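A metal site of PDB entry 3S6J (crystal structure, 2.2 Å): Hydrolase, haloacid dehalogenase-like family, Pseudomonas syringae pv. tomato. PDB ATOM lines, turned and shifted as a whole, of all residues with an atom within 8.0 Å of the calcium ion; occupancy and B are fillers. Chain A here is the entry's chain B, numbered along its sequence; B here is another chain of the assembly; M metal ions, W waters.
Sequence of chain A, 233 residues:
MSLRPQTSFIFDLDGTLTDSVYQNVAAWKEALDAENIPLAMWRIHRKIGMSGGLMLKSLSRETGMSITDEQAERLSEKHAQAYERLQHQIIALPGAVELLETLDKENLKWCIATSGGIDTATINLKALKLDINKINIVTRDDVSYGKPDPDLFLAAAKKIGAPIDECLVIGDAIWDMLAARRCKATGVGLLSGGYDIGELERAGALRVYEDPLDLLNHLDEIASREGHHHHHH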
ATOM      1  N   TYR A  22      18.049  -0.948   3.898  1.00  0.00           N
ATOM      2  CA  TYR A  22      17.243   0.254   4.071  1.00  0.00           C
ATOM      3  C   TYR A  22      17.745   1.122   5.259  1.00  0.00           C
ATOM      4  O   TYR A  22      17.744   2.340   5.194  1.00  0.00           O
ATOM      5  CB  TYR A  22      15.751  -0.084   4.173  1.00  0.00           C
ATOM      6  CG  TYR A  22      15.184  -0.617   2.854  1.00  0.00           C
ATOM      7  CD1 TYR A  22      14.330   0.161   2.073  1.00  0.00           C
ATOM      8  CD2 TYR A  22      15.511  -1.888   2.388  1.00  0.00           C
ATOM      9  CE1 TYR A  22      13.836  -0.318   0.866  1.00  0.00           C
ATOM     10  CE2 TYR A  22      15.010  -2.374   1.184  1.00  0.00           C
ATOM     11  CZ  TYR A  22      14.183  -1.585   0.421  1.00  0.00           C
ATOM     12  OH  TYR A  22      13.695  -2.054  -0.780  1.00  0.00           O
ATOM     13  N   TRP A  42      16.717   7.188  -3.608  1.00  0.00           N
ATOM     14  CA  TRP A  42      16.902   6.108  -4.585  1.00  0.00           C
ATOM     15  C   TRP A  42      18.326   6.067  -5.137  1.00  0.00           C
ATOM     16  O   TRP A  42      18.872   4.976  -5.381  1.00  0.00           O
ATOM     17  CB  TRP A  42      15.887   6.200  -5.707  1.00  0.00           C
ATOM     18  CG  TRP A  42      16.211   7.280  -6.711  1.00  0.00           C
ATOM     19  CD1 TRP A  42      15.917   8.596  -6.593  1.00  0.00           C
ATOM     20  CD2 TRP A  42      16.883   7.124  -7.960  1.00  0.00           C
ATOM     21  NE1 TRP A  42      16.364   9.277  -7.699  1.00  0.00           N
ATOM     22  CE2 TRP A  42      16.976   8.387  -8.562  1.00  0.00           C
ATOM     23  CE3 TRP A  42      17.417   6.031  -8.654  1.00  0.00           C
ATOM     24  CZ2 TRP A  42      17.549   8.616  -9.812  1.00  0.00           C
ATOM     25  CZ3 TRP A  42      18.027   6.244  -9.894  1.00  0.00           C
ATOM     26  CH2 TRP A  42      18.082   7.533 -10.455  1.00  0.00           C
ATOM     27  N   HIS A  45      20.443   4.336  -2.349  1.00  0.00           N
ATOM     28  CA  HIS A  45      20.118   2.917  -2.399  1.00  0.00           C
ATOM     29  C   HIS A  45      20.791   2.186  -3.588  1.00  0.00           C
ATOM     30  O   HIS A  45      21.261   1.050  -3.452  1.00  0.00           O
ATOM     31  CB  HIS A  45      18.596   2.770  -2.431  1.00  0.00           C
ATOM     32  CG  HIS A  45      18.117   1.365  -2.304  1.00  0.00           C
ATOM     33  ND1 HIS A  45      16.818   0.993  -2.559  1.00  0.00           N
ATOM     34  CD2 HIS A  45      18.767   0.221  -1.953  1.00  0.00           C
ATOM     35  CE1 HIS A  45      16.679  -0.304  -2.359  1.00  0.00           C
ATOM     36  NE2 HIS A  45      17.853  -0.794  -2.003  1.00  0.00           N
ATOM     37  N   ARG A  46      20.863   2.874  -4.728  1.00  0.00           N
ATOM     38  CA  ARG A  46      21.519   2.342  -5.919  1.00  0.00           C
ATOM     39  C   ARG A  46      22.981   2.051  -5.664  1.00  0.00           C
ATOM     40  O   ARG A  46      23.578   1.252  -6.394  1.00  0.00           O
ATOM     41  CB  ARG A  46      21.482   3.354  -7.085  1.00  0.00           C
ATOM     42  CG  ARG A  46      20.335   3.196  -8.062  1.00  0.00           C
ATOM     43  CD  ARG A  46      20.753   3.500  -9.527  1.00  0.00           C
ATOM     44  NE  ARG A  46      21.272   4.863  -9.755  1.00  0.00           N
ATOM     45  CZ  ARG A  46      21.300   5.463 -10.952  1.00  0.00           C
ATOM     46  NH1 ARG A  46      20.811   4.843 -12.031  1.00  0.00           N
ATOM     47  NH2 ARG A  46      21.796   6.688 -11.076  1.00  0.00           N
ATOM     48  N   LEU A 191      16.790 -10.606  -4.303  1.00  0.00           N
ATOM     49  CA  LEU A 191      15.948  -9.391  -4.442  1.00  0.00           C
ATOM     50  C   LEU A 191      15.886  -8.638  -3.121  1.00  0.00           C
ATOM     51  O   LEU A 191      15.267  -7.584  -3.020  1.00  0.00           O
ATOM     52  CB  LEU A 191      14.533  -9.770  -4.901  1.00  0.00           C
ATOM     53  CG  LEU A 191      14.449 -10.435  -6.286  1.00  0.00           C
ATOM     54  CD1 LEU A 191      13.056 -10.985  -6.645  1.00  0.00           C
ATOM     55  CD2 LEU A 191      14.957  -9.444  -7.369  1.00  0.00           C
ATOM     56  N   GLY A 193      17.847  -6.952  -1.338  1.00  0.00           N
ATOM     57  CA  GLY A 193      18.511  -5.665  -1.215  1.00  0.00           C
ATOM     58  C   GLY A 193      17.720  -4.545  -1.865  1.00  0.00           C
ATOM     59  O   GLY A 193      18.132  -3.384  -1.859  1.00  0.00           O
ATOM     60  N   GLY A 194      16.560  -4.880  -2.414  1.00  0.00           N
ATOM     61  CA  GLY A 194      15.766  -3.918  -3.152  1.00  0.00           C
ATOM     62  C   GLY A 194      16.169  -3.737  -4.622  1.00  0.00           C
ATOM     63  O   GLY A 194      15.587  -2.935  -5.301  1.00  0.00           O
ATOM     64  N   TYR A 195      17.194  -4.435  -5.102  1.00  0.00           N
ATOM     65  CA  TYR A 195      17.523  -4.319  -6.520  1.00  0.00           C
ATOM     66  C   TYR A 195      16.608  -5.312  -7.268  1.00  0.00           C
ATOM     67  O   TYR A 195      16.140  -6.312  -6.697  1.00  0.00           O
ATOM     68  CB  TYR A 195      19.004  -4.626  -6.806  1.00  0.00           C
ATOM     69  CG  TYR A 195      20.037  -3.655  -6.232  1.00  0.00           C
ATOM     70  CD1 TYR A 195      20.251  -3.547  -4.858  1.00  0.00           C
ATOM     71  CD2 TYR A 195      20.842  -2.884  -7.074  1.00  0.00           C
ATOM     72  CE1 TYR A 195      21.219  -2.666  -4.330  1.00  0.00           C
ATOM     73  CE2 TYR A 195      21.804  -2.007  -6.568  1.00  0.00           C
ATOM     74  CZ  TYR A 195      21.996  -1.899  -5.206  1.00  0.00           C
ATOM     75  OH  TYR A 195      22.958  -1.021  -4.700  1.00  0.00           O
ATOM     76  N   ASP A 196      16.365  -5.052  -8.530  1.00  0.00           N
ATOM     77  CA  ASP A 196      15.382  -5.855  -9.245  1.00  0.00           C
ATOM     78  C   ASP A 196      16.047  -6.919 -10.139  1.00  0.00           C
ATOM     79  O   ASP A 196      17.253  -6.844 -10.434  1.00  0.00           O
ATOM     80  CB  ASP A 196      14.434  -4.915 -10.012  1.00  0.00           C
ATOM     81  CG  ASP A 196      14.065  -3.669  -9.176  1.00  0.00           C
ATOM     82  OD1 ASP A 196      13.174  -3.765  -8.302  1.00  0.00           O
ATOM     83  OD2 ASP A 196      14.677  -2.592  -9.363  1.00  0.00           O
ATOM     84  N   ILE A 197      15.281  -7.925 -10.524  1.00  0.00           N
ATOM     85  CA  ILE A 197      15.823  -8.995 -11.343  1.00  0.00           C
ATOM     86  C   ILE A 197      16.595  -8.490 -12.602  1.00  0.00           C
ATOM     87  O   ILE A 197      17.702  -8.933 -12.904  1.00  0.00           O
ATOM     88  CB  ILE A 197      14.709  -9.979 -11.734  1.00  0.00           C
ATOM     89  CG1 ILE A 197      15.315 -11.223 -12.403  1.00  0.00           C
ATOM     90  CG2 ILE A 197      13.686  -9.290 -12.658  1.00  0.00           C
ATOM     91  CD1 ILE A 197      14.487 -12.491 -12.195  1.00  0.00           C
ATOM     92  N   GLU A 199      18.061  -5.504 -13.237  1.00  0.00           N
ATOM     93  CA  GLU A 199      19.306  -4.850 -12.848  1.00  0.00           C
ATOM     94  C   GLU A 199      20.383  -5.881 -12.545  1.00  0.00           C
ATOM     95  O   GLU A 199      21.507  -5.784 -13.036  1.00  0.00           O
ATOM     96  CB  GLU A 199      19.073  -4.056 -11.557  1.00  0.00           C
ATOM     97  CG  GLU A 199      18.721  -2.599 -11.684  1.00  0.00           C
ATOM     98  CD  GLU A 199      18.216  -2.031 -10.346  1.00  0.00           C
ATOM     99  OE1 GLU A 199      17.823  -2.842  -9.463  1.00  0.00           O
ATOM    100  OE2 GLU A 199      18.194  -0.784 -10.168  1.00  0.00           O
ATOM    101  N   TYR B  22      10.778   5.903   0.886  1.00  0.00           N
ATOM    102  CA  TYR B  22      11.586   5.241   1.909  1.00  0.00           C
ATOM    103  C   TYR B  22      11.006   5.463   3.309  1.00  0.00           C
ATOM    104  O   TYR B  22      11.044   4.566   4.145  1.00  0.00           O
ATOM    105  CB  TYR B  22      13.062   5.645   1.750  1.00  0.00           C
ATOM    106  CG  TYR B  22      13.637   5.062   0.469  1.00  0.00           C
ATOM    107  CD1 TYR B  22      14.421   3.917   0.501  1.00  0.00           C
ATOM    108  CD2 TYR B  22      13.350   5.620  -0.768  1.00  0.00           C
ATOM    109  CE1 TYR B  22      14.929   3.362  -0.675  1.00  0.00           C
ATOM    110  CE2 TYR B  22      13.850   5.075  -1.938  1.00  0.00           C
ATOM    111  CZ  TYR B  22      14.639   3.951  -1.883  1.00  0.00           C
ATOM    112  OH  TYR B  22      15.133   3.400  -3.050  1.00  0.00           O
ATOM    113  N   TRP B  42      12.225  -5.165   1.383  1.00  0.00           N
ATOM    114  CA  TRP B  42      12.066  -5.077  -0.066  1.00  0.00           C
ATOM    115  C   TRP B  42      10.636  -5.467  -0.453  1.00  0.00           C
ATOM    116  O   TRP B  42      10.073  -4.908  -1.388  1.00  0.00           O
ATOM    117  CB  TRP B  42      13.084  -5.949  -0.772  1.00  0.00           C
ATOM    118  CG  TRP B  42      12.813  -7.415  -0.580  1.00  0.00           C
ATOM    119  CD1 TRP B  42      13.071  -8.168   0.530  1.00  0.00           C
ATOM    120  CD2 TRP B  42      12.237  -8.313  -1.542  1.00  0.00           C
ATOM    121  NE1 TRP B  42      12.700  -9.475   0.330  1.00  0.00           N
ATOM    122  CE2 TRP B  42      12.173  -9.586  -0.933  1.00  0.00           C
ATOM    123  CE3 TRP B  42      11.753  -8.154  -2.841  1.00  0.00           C
ATOM    124  CZ2 TRP B  42      11.646 -10.710  -1.596  1.00  0.00           C
ATOM    125  CZ3 TRP B  42      11.246  -9.266  -3.498  1.00  0.00           C
ATOM    126  CH2 TRP B  42      11.202 -10.522  -2.874  1.00  0.00           C
ATOM    127  N   HIS B  45       8.500  -2.390   0.220  1.00  0.00           N
ATOM    128  CA  HIS B  45       8.848  -1.464  -0.837  1.00  0.00           C
ATOM    129  C   HIS B  45       8.100  -1.800  -2.131  1.00  0.00           C
ATOM    130  O   HIS B  45       7.528  -0.919  -2.782  1.00  0.00           O
ATOM    131  CB  HIS B  45      10.351  -1.519  -1.084  1.00  0.00           C
ATOM    132  CG  HIS B  45      10.868  -0.402  -1.940  1.00  0.00           C
ATOM    133  ND1 HIS B  45      12.213  -0.186  -2.143  1.00  0.00           N
ATOM    134  CD2 HIS B  45      10.226   0.583  -2.614  1.00  0.00           C
ATOM    135  CE1 HIS B  45      12.377   0.882  -2.911  1.00  0.00           C
ATOM    136  NE2 HIS B  45      11.182   1.353  -3.224  1.00  0.00           N
ATOM    137  N   ARG B  46       8.106  -3.079  -2.507  1.00  0.00           N
ATOM    138  CA  ARG B  46       7.442  -3.547  -3.740  1.00  0.00           C
ATOM    139  C   ARG B  46       5.964  -3.183  -3.775  1.00  0.00           C
ATOM    140  O   ARG B  46       5.359  -3.240  -4.834  1.00  0.00           O
ATOM    141  CB  ARG B  46       7.535  -5.067  -3.897  1.00  0.00           C
ATOM    142  CG  ARG B  46       8.631  -5.573  -4.844  1.00  0.00           C
ATOM    143  CD  ARG B  46       8.465  -7.094  -5.149  1.00  0.00           C
ATOM    144  NE  ARG B  46       7.809  -7.842  -4.063  1.00  0.00           N
ATOM    145  CZ  ARG B  46       7.570  -9.167  -4.078  1.00  0.00           C
ATOM    146  NH1 ARG B  46       7.937  -9.919  -5.114  1.00  0.00           N
ATOM    147  NH2 ARG B  46       6.964  -9.753  -3.051  1.00  0.00           N
ATOM    148  N   LEU B 191      12.366   6.613 -11.815  1.00  0.00           N
ATOM    149  CA  LEU B 191      13.207   5.792 -10.933  1.00  0.00           C
ATOM    150  C   LEU B 191      13.175   6.210  -9.461  1.00  0.00           C
ATOM    151  O   LEU B 191      13.614   5.457  -8.567  1.00  0.00           O
ATOM    152  CB  LEU B 191      14.654   5.814 -11.426  1.00  0.00           C
ATOM    153  CG  LEU B 191      14.797   5.298 -12.864  1.00  0.00           C
ATOM    154  CD1 LEU B 191      16.240   5.374 -13.317  1.00  0.00           C
ATOM    155  CD2 LEU B 191      14.251   3.883 -12.904  1.00  0.00           C
ATOM    156  N   GLY B 193      11.239   6.349  -7.015  1.00  0.00           N
ATOM    157  CA  GLY B 193      10.535   5.594  -5.984  1.00  0.00           C
ATOM    158  C   GLY B 193      11.246   4.272  -5.717  1.00  0.00           C
ATOM    159  O   GLY B 193      10.819   3.463  -4.904  1.00  0.00           O
ATOM    160  N   GLY B 194      12.335   4.056  -6.442  1.00  0.00           N
ATOM    161  CA  GLY B 194      13.167   2.883  -6.236  1.00  0.00           C
ATOM    162  C   GLY B 194      12.833   1.657  -7.084  1.00  0.00           C
ATOM    163  O   GLY B 194      13.436   0.641  -6.879  1.00  0.00           O
ATOM    164  N   TYR B 195      11.863   1.740  -7.996  1.00  0.00           N
ATOM    165  CA  TYR B 195      11.681   0.649  -8.963  1.00  0.00           C
ATOM    166  C   TYR B 195      12.674   0.796 -10.117  1.00  0.00           C
ATOM    167  O   TYR B 195      13.166   1.891 -10.398  1.00  0.00           O
ATOM    168  CB  TYR B 195      10.241   0.628  -9.484  1.00  0.00           C
ATOM    169  CG  TYR B 195       9.178   0.356  -8.428  1.00  0.00           C
ATOM    170  CD1 TYR B 195       8.873   1.296  -7.464  1.00  0.00           C
ATOM    171  CD2 TYR B 195       8.471  -0.850  -8.404  1.00  0.00           C
ATOM    172  CE1 TYR B 195       7.916   1.059  -6.487  1.00  0.00           C
ATOM    173  CE2 TYR B 195       7.494  -1.103  -7.442  1.00  0.00           C
ATOM    174  CZ  TYR B 195       7.216  -0.136  -6.490  1.00  0.00           C
ATOM    175  OH  TYR B 195       6.258  -0.356  -5.512  1.00  0.00           O
ATOM    176  N   ASP B 196      12.996  -0.299 -10.797  1.00  0.00           N
ATOM    177  CA  ASP B 196      13.986  -0.238 -11.884  1.00  0.00           C
ATOM    178  C   ASP B 196      13.298  -0.082 -13.248  1.00  0.00           C
ATOM    179  O   ASP B 196      12.092  -0.270 -13.357  1.00  0.00           O
ATOM    180  CB  ASP B 196      14.937  -1.453 -11.864  1.00  0.00           C
ATOM    181  CG  ASP B 196      14.536  -2.566 -12.841  1.00  0.00           C
ATOM    182  OD1 ASP B 196      13.542  -3.274 -12.570  1.00  0.00           O
ATOM    183  OD2 ASP B 196      15.241  -2.762 -13.877  1.00  0.00           O
ATOM    184  N   ILE B 197      14.063   0.302 -14.265  1.00  0.00           N
ATOM    185  CA  ILE B 197      13.481   0.577 -15.562  1.00  0.00           C
ATOM    186  C   ILE B 197      12.723  -0.651 -16.114  1.00  0.00           C
ATOM    187  O   ILE B 197      11.601  -0.530 -16.603  1.00  0.00           O
ATOM    188  CB  ILE B 197      14.543   1.103 -16.558  1.00  0.00           C
ATOM    189  CG1 ILE B 197      13.923   1.318 -17.938  1.00  0.00           C
ATOM    190  CG2 ILE B 197      15.709   0.142 -16.681  1.00  0.00           C
ATOM    191  CD1 ILE B 197      14.724   2.285 -18.814  1.00  0.00           C
ATOM    192  N   GLU B 199      11.294  -3.267 -14.508  1.00  0.00           N
ATOM    193  CA  GLU B 199      10.034  -3.429 -13.776  1.00  0.00           C
ATOM    194  C   GLU B 199       8.981  -2.479 -14.330  1.00  0.00           C
ATOM    195  O   GLU B 199       7.831  -2.853 -14.587  1.00  0.00           O
ATOM    196  CB  GLU B 199      10.198  -3.126 -12.281  1.00  0.00           C
ATOM    197  CG  GLU B 199      10.610  -4.275 -11.364  1.00  0.00           C
ATOM    198  CD  GLU B 199      10.837  -3.798  -9.909  1.00  0.00           C
ATOM    199  OE1 GLU B 199      10.814  -2.566  -9.667  1.00  0.00           O
ATOM    200  OE2 GLU B 199      11.041  -4.653  -9.007  1.00  0.00           O
HETATM  201 CA    CA M   1      14.566  -1.434  -6.734  1.00  0.00          CA
HETATM  202  O   HOH W   1      17.355  -0.384  -7.341  1.00  0.00           O
HETATM  203  O   HOH W   2      16.275   0.027  -5.241  1.00  0.00           O
HETATM  204  O   HOH W   3      11.885  -2.540  -6.429  1.00  0.00           O
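The side-chain carboxylate (OE1) of Glu 199 of chain A lies within hydrogen-bond range of the backbone NH (N) of Asp 196 of chain A (2.8 Å).
The backbone NH (N) of Asp 196 of chain B lies close to the side-chain carboxylate (OD2) of Asp 196 of chain A (3.2 Å).
OE2 of Glu 199 of chain B sits close to OD1 of Asp 196 of chain A.
Within 4 Å of the calcium ion: Gly 194 of chain A, Asp 196 of chain A and Gly 194 of chain B.
Along chain A the residues within 4 Å of the calcium ion span positions 194 to 196.
The nearest printed residue that does not touch the calcium ion is Tyr 195 of chain A (4.1 Å).
The calcium ion is bound by the backbone carbonyl oxygen of Gly 194 of chain A (2.3 Å), the backbone carbonyl oxygen of Gly 194 of chain B (2.4 Å), water W2 (2.7 Å) and the side-chain carboxylate of Asp 196 of chain A (2.9 Å).
Slightly farther from the calcium ion lies water W3 (2.9 Å).
Slightly farther from the calcium ion lies water W1 (3.0 Å).
Slightly farther from the calcium ion lies OD1 of Asp 196 of chain A (3.1 Å).
Water W3 lies within hydrogen-bond range of OD1 of Asp 196 of chain A and OE1 of Glu 199 of chain B.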
